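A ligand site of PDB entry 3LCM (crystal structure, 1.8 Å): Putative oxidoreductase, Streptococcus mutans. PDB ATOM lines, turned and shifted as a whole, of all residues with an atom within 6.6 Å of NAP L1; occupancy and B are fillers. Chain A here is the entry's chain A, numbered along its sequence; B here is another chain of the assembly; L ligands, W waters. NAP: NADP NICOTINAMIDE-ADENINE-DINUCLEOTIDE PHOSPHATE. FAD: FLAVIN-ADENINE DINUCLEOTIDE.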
ATOM      1  N   ARG A  55     -20.486   5.852  16.094  1.00  0.00           N
ATOM      2  CA  ARG A  55     -21.873   6.237  16.181  1.00  0.00           C
ATOM      3  C   ARG A  55     -22.506   6.273  14.799  1.00  0.00           C
ATOM      4  O   ARG A  55     -23.649   5.905  14.640  1.00  0.00           O
ATOM      5  CB  ARG A  55     -21.971   7.596  16.813  1.00  0.00           C
ATOM      6  CG  ARG A  55     -23.311   8.042  17.095  1.00  0.00           C
ATOM      7  CD  ARG A  55     -23.342   9.400  17.599  1.00  0.00           C
ATOM      8  NE  ARG A  55     -24.627  10.051  17.385  1.00  0.00           N
ATOM      9  CZ  ARG A  55     -24.891  11.316  17.657  1.00  0.00           C
ATOM     10  NH1 ARG A  55     -26.105  11.790  17.443  1.00  0.00           N
ATOM     11  NH2 ARG A  55     -23.976  12.121  18.160  1.00  0.00           N
ATOM     12  N   PHE A 100     -34.080   3.361  17.050  1.00  0.00           N
ATOM     13  CA  PHE A 100     -34.491   4.588  16.386  1.00  0.00           C
ATOM     14  C   PHE A 100     -33.280   5.499  16.180  1.00  0.00           C
ATOM     15  O   PHE A 100     -33.177   6.559  16.816  1.00  0.00           O
ATOM     16  CB  PHE A 100     -35.588   5.297  17.184  1.00  0.00           C
ATOM     17  CG  PHE A 100     -36.944   4.636  17.084  1.00  0.00           C
ATOM     18  CD1 PHE A 100     -37.108   3.301  17.483  1.00  0.00           C
ATOM     19  CD2 PHE A 100     -38.045   5.332  16.611  1.00  0.00           C
ATOM     20  CE1 PHE A 100     -38.345   2.682  17.395  1.00  0.00           C
ATOM     21  CE2 PHE A 100     -39.288   4.710  16.507  1.00  0.00           C
ATOM     22  CZ  PHE A 100     -39.430   3.386  16.909  1.00  0.00           C
ATOM     23  N   ALA A 102     -30.133   7.541  13.737  1.00  0.00           N
ATOM     24  CA  ALA A 102     -29.968   8.357  12.543  1.00  0.00           C
ATOM     25  C   ALA A 102     -29.698   7.479  11.318  1.00  0.00           C
ATOM     26  O   ALA A 102     -29.030   6.450  11.424  1.00  0.00           O
ATOM     27  CB  ALA A 102     -28.839   9.349  12.728  1.00  0.00           C
ATOM     28  N   TYR A 106     -34.612   8.652  11.388  1.00  0.00           N
ATOM     29  CA  TYR A 106     -34.502  10.076  11.120  1.00  0.00           C
ATOM     30  C   TYR A 106     -33.120  10.406  10.520  1.00  0.00           C
ATOM     31  O   TYR A 106     -32.186   9.608  10.605  1.00  0.00           O
ATOM     32  CB  TYR A 106     -34.699  10.879  12.410  1.00  0.00           C
ATOM     33  CG  TYR A 106     -33.535  10.756  13.372  1.00  0.00           C
ATOM     34  CD1 TYR A 106     -33.507   9.750  14.334  1.00  0.00           C
ATOM     35  CD2 TYR A 106     -32.454  11.627  13.306  1.00  0.00           C
ATOM     36  CE1 TYR A 106     -32.440   9.616  15.201  1.00  0.00           C
ATOM     37  CE2 TYR A 106     -31.371  11.500  14.159  1.00  0.00           C
ATOM     38  CZ  TYR A 106     -31.374  10.493  15.120  1.00  0.00           C
ATOM     39  OH  TYR A 106     -30.307  10.359  15.987  1.00  0.00           O
ATOM     40  N   TYR A 108     -30.580  14.270   9.499  1.00  0.00           N
ATOM     41  CA  TYR A 108     -30.464  15.697   9.763  1.00  0.00           C
ATOM     42  C   TYR A 108     -30.728  16.518   8.509  1.00  0.00           C
ATOM     43  O   TYR A 108     -30.143  16.274   7.444  1.00  0.00           O
ATOM     44  CB  TYR A 108     -29.085  16.002  10.351  1.00  0.00           C
ATOM     45  CG  TYR A 108     -28.707  15.061  11.472  1.00  0.00           C
ATOM     46  CD1 TYR A 108     -28.052  13.868  11.212  1.00  0.00           C
ATOM     47  CD2 TYR A 108     -29.045  15.349  12.798  1.00  0.00           C
ATOM     48  CE1 TYR A 108     -27.714  12.989  12.227  1.00  0.00           C
ATOM     49  CE2 TYR A 108     -28.707  14.479  13.818  1.00  0.00           C
ATOM     50  CZ  TYR A 108     -28.042  13.308  13.537  1.00  0.00           C
ATOM     51  OH  TYR A 108     -27.699  12.433  14.545  1.00  0.00           O
ATOM     52  N   LEU A 113     -34.528  18.095  11.882  1.00  0.00           N
ATOM     53  CA  LEU A 113     -34.474  16.665  11.592  1.00  0.00           C
ATOM     54  C   LEU A 113     -35.550  16.362  10.569  1.00  0.00           C
ATOM     55  O   LEU A 113     -36.575  17.040  10.540  1.00  0.00           O
ATOM     56  CB  LEU A 113     -34.768  15.830  12.841  1.00  0.00           C
ATOM     57  CG  LEU A 113     -33.888  15.896  14.080  1.00  0.00           C
ATOM     58  CD1 LEU A 113     -34.417  14.904  15.112  1.00  0.00           C
ATOM     59  CD2 LEU A 113     -32.423  15.593  13.743  1.00  0.00           C
ATOM     60  N   GLN A 148     -41.858  14.077  21.421  1.00  0.00           N
ATOM     61  CA  GLN A 148     -40.434  14.331  21.221  1.00  0.00           C
ATOM     62  C   GLN A 148     -39.640  13.131  20.715  1.00  0.00           C
ATOM     63  O   GLN A 148     -38.426  13.228  20.526  1.00  0.00           O
ATOM     64  CB  GLN A 148     -39.825  14.957  22.487  1.00  0.00           C
ATOM     65  CG  GLN A 148     -40.324  16.387  22.708  1.00  0.00           C
ATOM     66  CD  GLN A 148     -39.952  16.966  24.053  1.00  0.00           C
ATOM     67  OE1 GLN A 148     -40.643  17.854  24.563  1.00  0.00           O
ATOM     68  NE2 GLN A 148     -38.873  16.468  24.642  1.00  0.00           N
ATOM     69  N   PRO A 152     -41.179  13.446  15.905  1.00  0.00           N
ATOM     70  CA  PRO A 152     -40.037  13.887  15.092  1.00  0.00           C
ATOM     71  C   PRO A 152     -39.589  12.853  14.055  1.00  0.00           C
ATOM     72  O   PRO A 152     -38.969  13.235  13.060  1.00  0.00           O
ATOM     73  CB  PRO A 152     -38.936  14.123  16.139  1.00  0.00           C
ATOM     74  CG  PRO A 152     -39.676  14.423  17.395  1.00  0.00           C
ATOM     75  CD  PRO A 152     -40.917  13.582  17.349  1.00  0.00           C
ATOM     76  N   ILE B  83     -28.054  14.127  26.828  1.00  0.00           N
ATOM     77  CA  ILE B  83     -29.472  13.939  26.583  1.00  0.00           C
ATOM     78  C   ILE B  83     -29.659  13.001  25.385  1.00  0.00           C
ATOM     79  O   ILE B  83     -29.220  13.316  24.267  1.00  0.00           O
ATOM     80  CB  ILE B  83     -30.167  15.275  26.287  1.00  0.00           C
ATOM     81  CG1 ILE B  83     -30.179  16.157  27.541  1.00  0.00           C
ATOM     82  CG2 ILE B  83     -31.576  15.048  25.786  1.00  0.00           C
ATOM     83  CD1 ILE B  83     -30.888  15.534  28.721  1.00  0.00           C
ATOM     84  N   TRP B  84     -30.272  11.850  25.615  1.00  0.00           N
ATOM     85  CA  TRP B  84     -30.683  10.953  24.522  1.00  0.00           C
ATOM     86  C   TRP B  84     -32.188  10.860  24.506  1.00  0.00           C
ATOM     87  O   TRP B  84     -32.806  10.407  25.465  1.00  0.00           O
ATOM     88  CB  TRP B  84     -30.099   9.542  24.648  1.00  0.00           C
ATOM     89  CG  TRP B  84     -28.622   9.460  24.430  1.00  0.00           C
ATOM     90  CD1 TRP B  84     -27.788  10.459  24.025  1.00  0.00           C
ATOM     91  CD2 TRP B  84     -27.800   8.296  24.592  1.00  0.00           C
ATOM     92  NE1 TRP B  84     -26.486  10.004  23.938  1.00  0.00           N
ATOM     93  CE2 TRP B  84     -26.470   8.669  24.281  1.00  0.00           C
ATOM     94  CE3 TRP B  84     -28.060   6.978  24.995  1.00  0.00           C
ATOM     95  CZ2 TRP B  84     -25.405   7.773  24.347  1.00  0.00           C
ATOM     96  CZ3 TRP B  84     -27.001   6.087  25.050  1.00  0.00           C
ATOM     97  CH2 TRP B  84     -25.686   6.486  24.733  1.00  0.00           C
ATOM     98  N   TRP B  85     -32.786  11.267  23.390  1.00  0.00           N
ATOM     99  CA  TRP B  85     -34.240  11.292  23.276  1.00  0.00           C
ATOM    100  C   TRP B  85     -34.890  11.992  24.476  1.00  0.00           C
ATOM    101  O   TRP B  85     -35.768  11.439  25.128  1.00  0.00           O
ATOM    102  CB  TRP B  85     -34.798   9.885  23.061  1.00  0.00           C
ATOM    103  CG  TRP B  85     -34.361   9.298  21.756  1.00  0.00           C
ATOM    104  CD1 TRP B  85     -33.466   8.292  21.561  1.00  0.00           C
ATOM    105  CD2 TRP B  85     -34.782   9.726  20.450  1.00  0.00           C
ATOM    106  NE1 TRP B  85     -33.308   8.042  20.214  1.00  0.00           N
ATOM    107  CE2 TRP B  85     -34.102   8.915  19.518  1.00  0.00           C
ATOM    108  CE3 TRP B  85     -35.663  10.704  19.987  1.00  0.00           C
ATOM    109  CZ2 TRP B  85     -34.283   9.043  18.136  1.00  0.00           C
ATOM    110  CZ3 TRP B  85     -35.848  10.836  18.618  1.00  0.00           C
ATOM    111  CH2 TRP B  85     -35.157  10.014  17.709  1.00  0.00           C
ATOM    112  N   SER B  86     -34.413  13.202  24.747  1.00  0.00           N
ATOM    113  CA  SER B  86     -35.006  14.117  25.722  1.00  0.00           C
ATOM    114  C   SER B  86     -34.679  13.761  27.169  1.00  0.00           C
ATOM    115  O   SER B  86     -35.138  14.429  28.085  1.00  0.00           O
ATOM    116  CB  SER B  86     -36.521  14.212  25.533  1.00  0.00           C
ATOM    117  OG  SER B  86     -36.808  14.685  24.235  1.00  0.00           O
ATOM    118  N   ASN B 129     -27.962  18.991  21.922  1.00  0.00           N
ATOM    119  CA  ASN B 129     -27.756  19.796  20.728  1.00  0.00           C
ATOM    120  C   ASN B 129     -28.924  20.750  20.430  1.00  0.00           C
ATOM    121  O   ASN B 129     -29.051  21.263  19.330  1.00  0.00           O
ATOM    122  CB  ASN B 129     -27.421  18.900  19.521  1.00  0.00           C
ATOM    123  CG  ASN B 129     -26.591  19.621  18.465  1.00  0.00           C
ATOM    124  OD1 ASN B 129     -25.879  20.581  18.757  1.00  0.00           O
ATOM    125  ND2 ASN B 129     -26.684  19.154  17.225  1.00  0.00           N
ATOM    126  N   THR B 130     -29.757  21.010  21.447  1.00  0.00           N
ATOM    127  CA  THR B 130     -30.907  21.916  21.290  1.00  0.00           C
ATOM    128  C   THR B 130     -30.555  23.322  21.788  1.00  0.00           C
ATOM    129  O   THR B 130     -29.981  23.470  22.867  1.00  0.00           O
ATOM    130  CB  THR B 130     -32.156  21.393  22.039  1.00  0.00           C
ATOM    131  OG1 THR B 130     -32.566  20.132  21.494  1.00  0.00           O
ATOM    132  CG2 THR B 130     -33.314  22.388  21.972  1.00  0.00           C
ATOM    133  N   TYR B 141     -35.360  16.797  29.398  1.00  0.00           N
ATOM    134  CA  TYR B 141     -34.012  17.345  29.232  1.00  0.00           C
ATOM    135  C   TYR B 141     -33.316  17.578  30.574  1.00  0.00           C
ATOM    136  O   TYR B 141     -32.641  18.590  30.781  1.00  0.00           O
ATOM    137  CB  TYR B 141     -34.040  18.645  28.421  1.00  0.00           C
ATOM    138  CG  TYR B 141     -34.061  18.461  26.911  1.00  0.00           C
ATOM    139  CD1 TYR B 141     -32.965  18.835  26.140  1.00  0.00           C
ATOM    140  CD2 TYR B 141     -35.179  17.941  26.252  1.00  0.00           C
ATOM    141  CE1 TYR B 141     -32.964  18.684  24.765  1.00  0.00           C
ATOM    142  CE2 TYR B 141     -35.187  17.783  24.869  1.00  0.00           C
ATOM    143  CZ  TYR B 141     -34.080  18.164  24.130  1.00  0.00           C
ATOM    144  OH  TYR B 141     -34.079  18.022  22.759  1.00  0.00           O
ATOM    145  N   GLU B 167     -23.069  20.376  19.778  1.00  0.00           N
ATOM    146  CA  GLU B 167     -22.388  19.857  18.599  1.00  0.00           C
ATOM    147  C   GLU B 167     -22.324  20.900  17.480  1.00  0.00           C
ATOM    148  O   GLU B 167     -21.488  20.803  16.584  1.00  0.00           O
ATOM    149  CB  GLU B 167     -23.030  18.535  18.140  1.00  0.00           C
ATOM    150  CG  GLU B 167     -22.713  17.399  19.111  1.00  0.00           C
ATOM    151  CD  GLU B 167     -23.647  16.225  18.964  1.00  0.00           C
ATOM    152  OE1 GLU B 167     -24.856  16.432  18.747  1.00  0.00           O
ATOM    153  OE2 GLU B 167     -23.166  15.068  19.092  1.00  0.00           O
HETATM  154  N1N NAP L   1     -32.948  14.821  18.785  1.00  0.00           N
HETATM  155  C2N NAP L   1     -31.643  14.912  18.367  1.00  0.00           C
HETATM  156  C3N NAP L   1     -30.909  13.736  17.920  1.00  0.00           C
HETATM  157  C7N NAP L   1     -29.445  13.772  17.421  1.00  0.00           C
HETATM  158  O7N NAP L   1     -28.674  14.623  17.621  1.00  0.00           O
HETATM  159  N7N NAP L   1     -29.002  12.664  16.644  1.00  0.00           N
HETATM  160  C4N NAP L   1     -31.602  12.508  17.920  1.00  0.00           C
HETATM  161  C5N NAP L   1     -32.919  12.424  18.434  1.00  0.00           C
HETATM  162  C6N NAP L   1     -33.627  13.594  18.804  1.00  0.00           C
HETATM  163  PA  FAD L   2     -19.225  13.781  21.470  1.00  0.00           P
HETATM  164  O1A FAD L   2     -19.764  13.161  20.129  1.00  0.00           O
HETATM  165  O2A FAD L   2     -18.241  12.985  22.022  1.00  0.00           O
HETATM  166  O5B FAD L   2     -18.437  15.084  21.081  1.00  0.00           O
HETATM  167  C5B FAD L   2     -19.179  16.171  20.721  1.00  0.00           C
HETATM  168  C4B FAD L   2     -18.304  17.273  20.181  1.00  0.00           C
HETATM  169  O4B FAD L   2     -17.384  17.798  21.131  1.00  0.00           O
HETATM  170  C3B FAD L   2     -17.403  16.896  18.953  1.00  0.00           C
HETATM  171  O3B FAD L   2     -17.443  17.793  17.918  1.00  0.00           O
HETATM  172  C2B FAD L   2     -16.063  16.613  19.619  1.00  0.00           C
HETATM  173  O2B FAD L   2     -14.930  16.349  18.873  1.00  0.00           O
HETATM  174  C1B FAD L   2     -16.102  17.691  20.637  1.00  0.00           C
HETATM  175  N9A FAD L   2     -15.100  17.557  21.657  1.00  0.00           N
HETATM  176  C8A FAD L   2     -14.759  16.448  22.327  1.00  0.00           C
HETATM  177  N7A FAD L   2     -13.769  16.785  23.210  1.00  0.00           N
HETATM  178  C5A FAD L   2     -13.506  18.112  23.078  1.00  0.00           C
HETATM  179  C6A FAD L   2     -12.709  18.968  23.784  1.00  0.00           C
HETATM  180  N6A FAD L   2     -11.722  18.482  24.701  1.00  0.00           N
HETATM  181  N1A FAD L   2     -12.595  20.231  23.436  1.00  0.00           N
HETATM  182  C2A FAD L   2     -13.456  20.685  22.544  1.00  0.00           C
HETATM  183  N3A FAD L   2     -14.360  19.890  21.955  1.00  0.00           N
HETATM  184  C4A FAD L   2     -14.315  18.601  22.142  1.00  0.00           C
HETATM  185  N1  FAD L   2     -29.703  15.999  21.338  1.00  0.00           N
HETATM  186  C2  FAD L   2     -30.907  16.882  21.447  1.00  0.00           C
HETATM  187  O2  FAD L   2     -30.736  18.165  21.709  1.00  0.00           O
HETATM  188  N3  FAD L   2     -32.124  16.208  22.073  1.00  0.00           N
HETATM  189  C4  FAD L   2     -32.476  14.723  21.846  1.00  0.00           C
HETATM  190  O4  FAD L   2     -33.511  14.180  22.557  1.00  0.00           O
HETATM  191  C4X FAD L   2     -31.239  13.880  21.568  1.00  0.00           C
HETATM  192  N5  FAD L   2     -31.272  12.442  21.489  1.00  0.00           N
HETATM  193  C5X FAD L   2     -30.095  11.734  21.074  1.00  0.00           C
HETATM  194  C6  FAD L   2     -30.167  10.360  21.132  1.00  0.00           C
HETATM  195  C7  FAD L   2     -29.140   9.571  20.804  1.00  0.00           C
HETATM  196  C7M FAD L   2     -29.310   8.081  20.820  1.00  0.00           C
HETATM  197  C8  FAD L   2     -27.957  10.141  20.628  1.00  0.00           C
HETATM  198  C8M FAD L   2     -26.734   9.273  20.379  1.00  0.00           C
HETATM  199  C9  FAD L   2     -27.856  11.487  20.628  1.00  0.00           C
HETATM  200  C9A FAD L   2     -28.957  12.302  20.901  1.00  0.00           C
HETATM  201  N10 FAD L   2     -28.788  13.686  20.939  1.00  0.00           N
HETATM  202  C10 FAD L   2     -29.903  14.540  21.178  1.00  0.00           C
HETATM  203  C1' FAD L   2     -27.494  14.338  20.875  1.00  0.00           C
HETATM  204  C2' FAD L   2     -26.722  14.236  22.198  1.00  0.00           C
HETATM  205  O2' FAD L   2     -27.294  14.797  23.300  1.00  0.00           O
HETATM  206  C3' FAD L   2     -25.274  14.626  22.017  1.00  0.00           C
HETATM  207  O3' FAD L   2     -24.694  13.934  21.020  1.00  0.00           O
HETATM  208  C4' FAD L   2     -24.525  14.793  23.336  1.00  0.00           C
HETATM  209  O4' FAD L   2     -25.081  15.671  24.187  1.00  0.00           O
HETATM  210  C5' FAD L   2     -23.061  15.105  23.135  1.00  0.00           C
HETATM  211  O5' FAD L   2     -22.147  14.638  24.054  1.00  0.00           O
HETATM  212  P   FAD L   2     -21.053  13.538  23.680  1.00  0.00           P
HETATM  213  O1P FAD L   2     -20.007  13.457  24.842  1.00  0.00           O
HETATM  214  O2P FAD L   2     -21.604  12.404  23.163  1.00  0.00           O
HETATM  215  O3P FAD L   2     -20.336  14.261  22.457  1.00  0.00           O
HETATM  216  O   HOH W   1     -26.189  14.574  17.441  1.00  0.00           O
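An oxygen (O3') of FAD L2 sits at hydrogen-bond distance from the side-chain carboxylate (OE2) of Glu 167 of chain B.
The backbone NH (N) of Ser 86 of chain B lies within hydrogen-bond range of an oxygen (O4) of FAD L2 (2.6 Å).
A nitrogen (N7N) of NAP L1 lies within hydrogen-bond range of the side-chain hydroxyl (OH) of Tyr 106 (2.7 Å).
OG1 of Thr 130 of chain B lies within hydrogen-bond range of O2 of FAD L2 (2.7 Å).
The side-chain hydroxyl of Tyr 108 is in hydrogen-bond range of a nitrogen (N7N) of NAP L1, 2.5 Å away.
An oxygen (O2') of FAD L2 lies within hydrogen-bond range of the backbone carbonyl oxygen (O) of Ile 83 of chain B, at 2.6 Å.
A nitrogen (N5) of FAD L2 sits at hydrogen-bond distance from the backbone NH of Trp 85 of chain B, at 2.7 Å.
N of Asn 129 of chain B lies within hydrogen-bond range of O2 of FAD L2 (2.9 Å).
OH of Tyr 141 of chain B lies within hydrogen-bond range of N3 of FAD L2 (2.8 Å).
O2 of FAD L2 lies within hydrogen-bond range of N of Thr 130 of chain B (3.0 Å).
An oxygen (O3') of FAD L2 sits at hydrogen-bond distance from the guanidinium group (NH2) of Arg 55.
Water W1 lies within hydrogen-bond range of an oxygen (O7N) of NAP L1 (2.5 Å), the side-chain carboxylate (OE1) of Glu 167 of chain B (2.6 Å) and the guanidinium group (NH1) of Arg 55 (2.8 Å).
OE2 of Glu 167 of chain B is in salt-bridge range of NH2 of Arg 55.
The side-chain hydroxyl of Tyr 108 lies within hydrogen-bond range of the guanidinium group of Arg 55 (3.4 Å).
NH1 of Arg 55 lies close to N7N of NAP L1, 3.1 Å away.
CD1 of Leu 113 touches N1N of NAP L1, 3.96 Å away.
Trp 85 of chain B touches NAP L1.
Hydrophobic or aromatic side chains that line NAP L1: Tyr 106, Tyr 108, Leu 113 and Trp 85 of chain B.
The nearest printed residue that does not touch NAP L1 is Glu 167 of chain B (4.4 Å).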
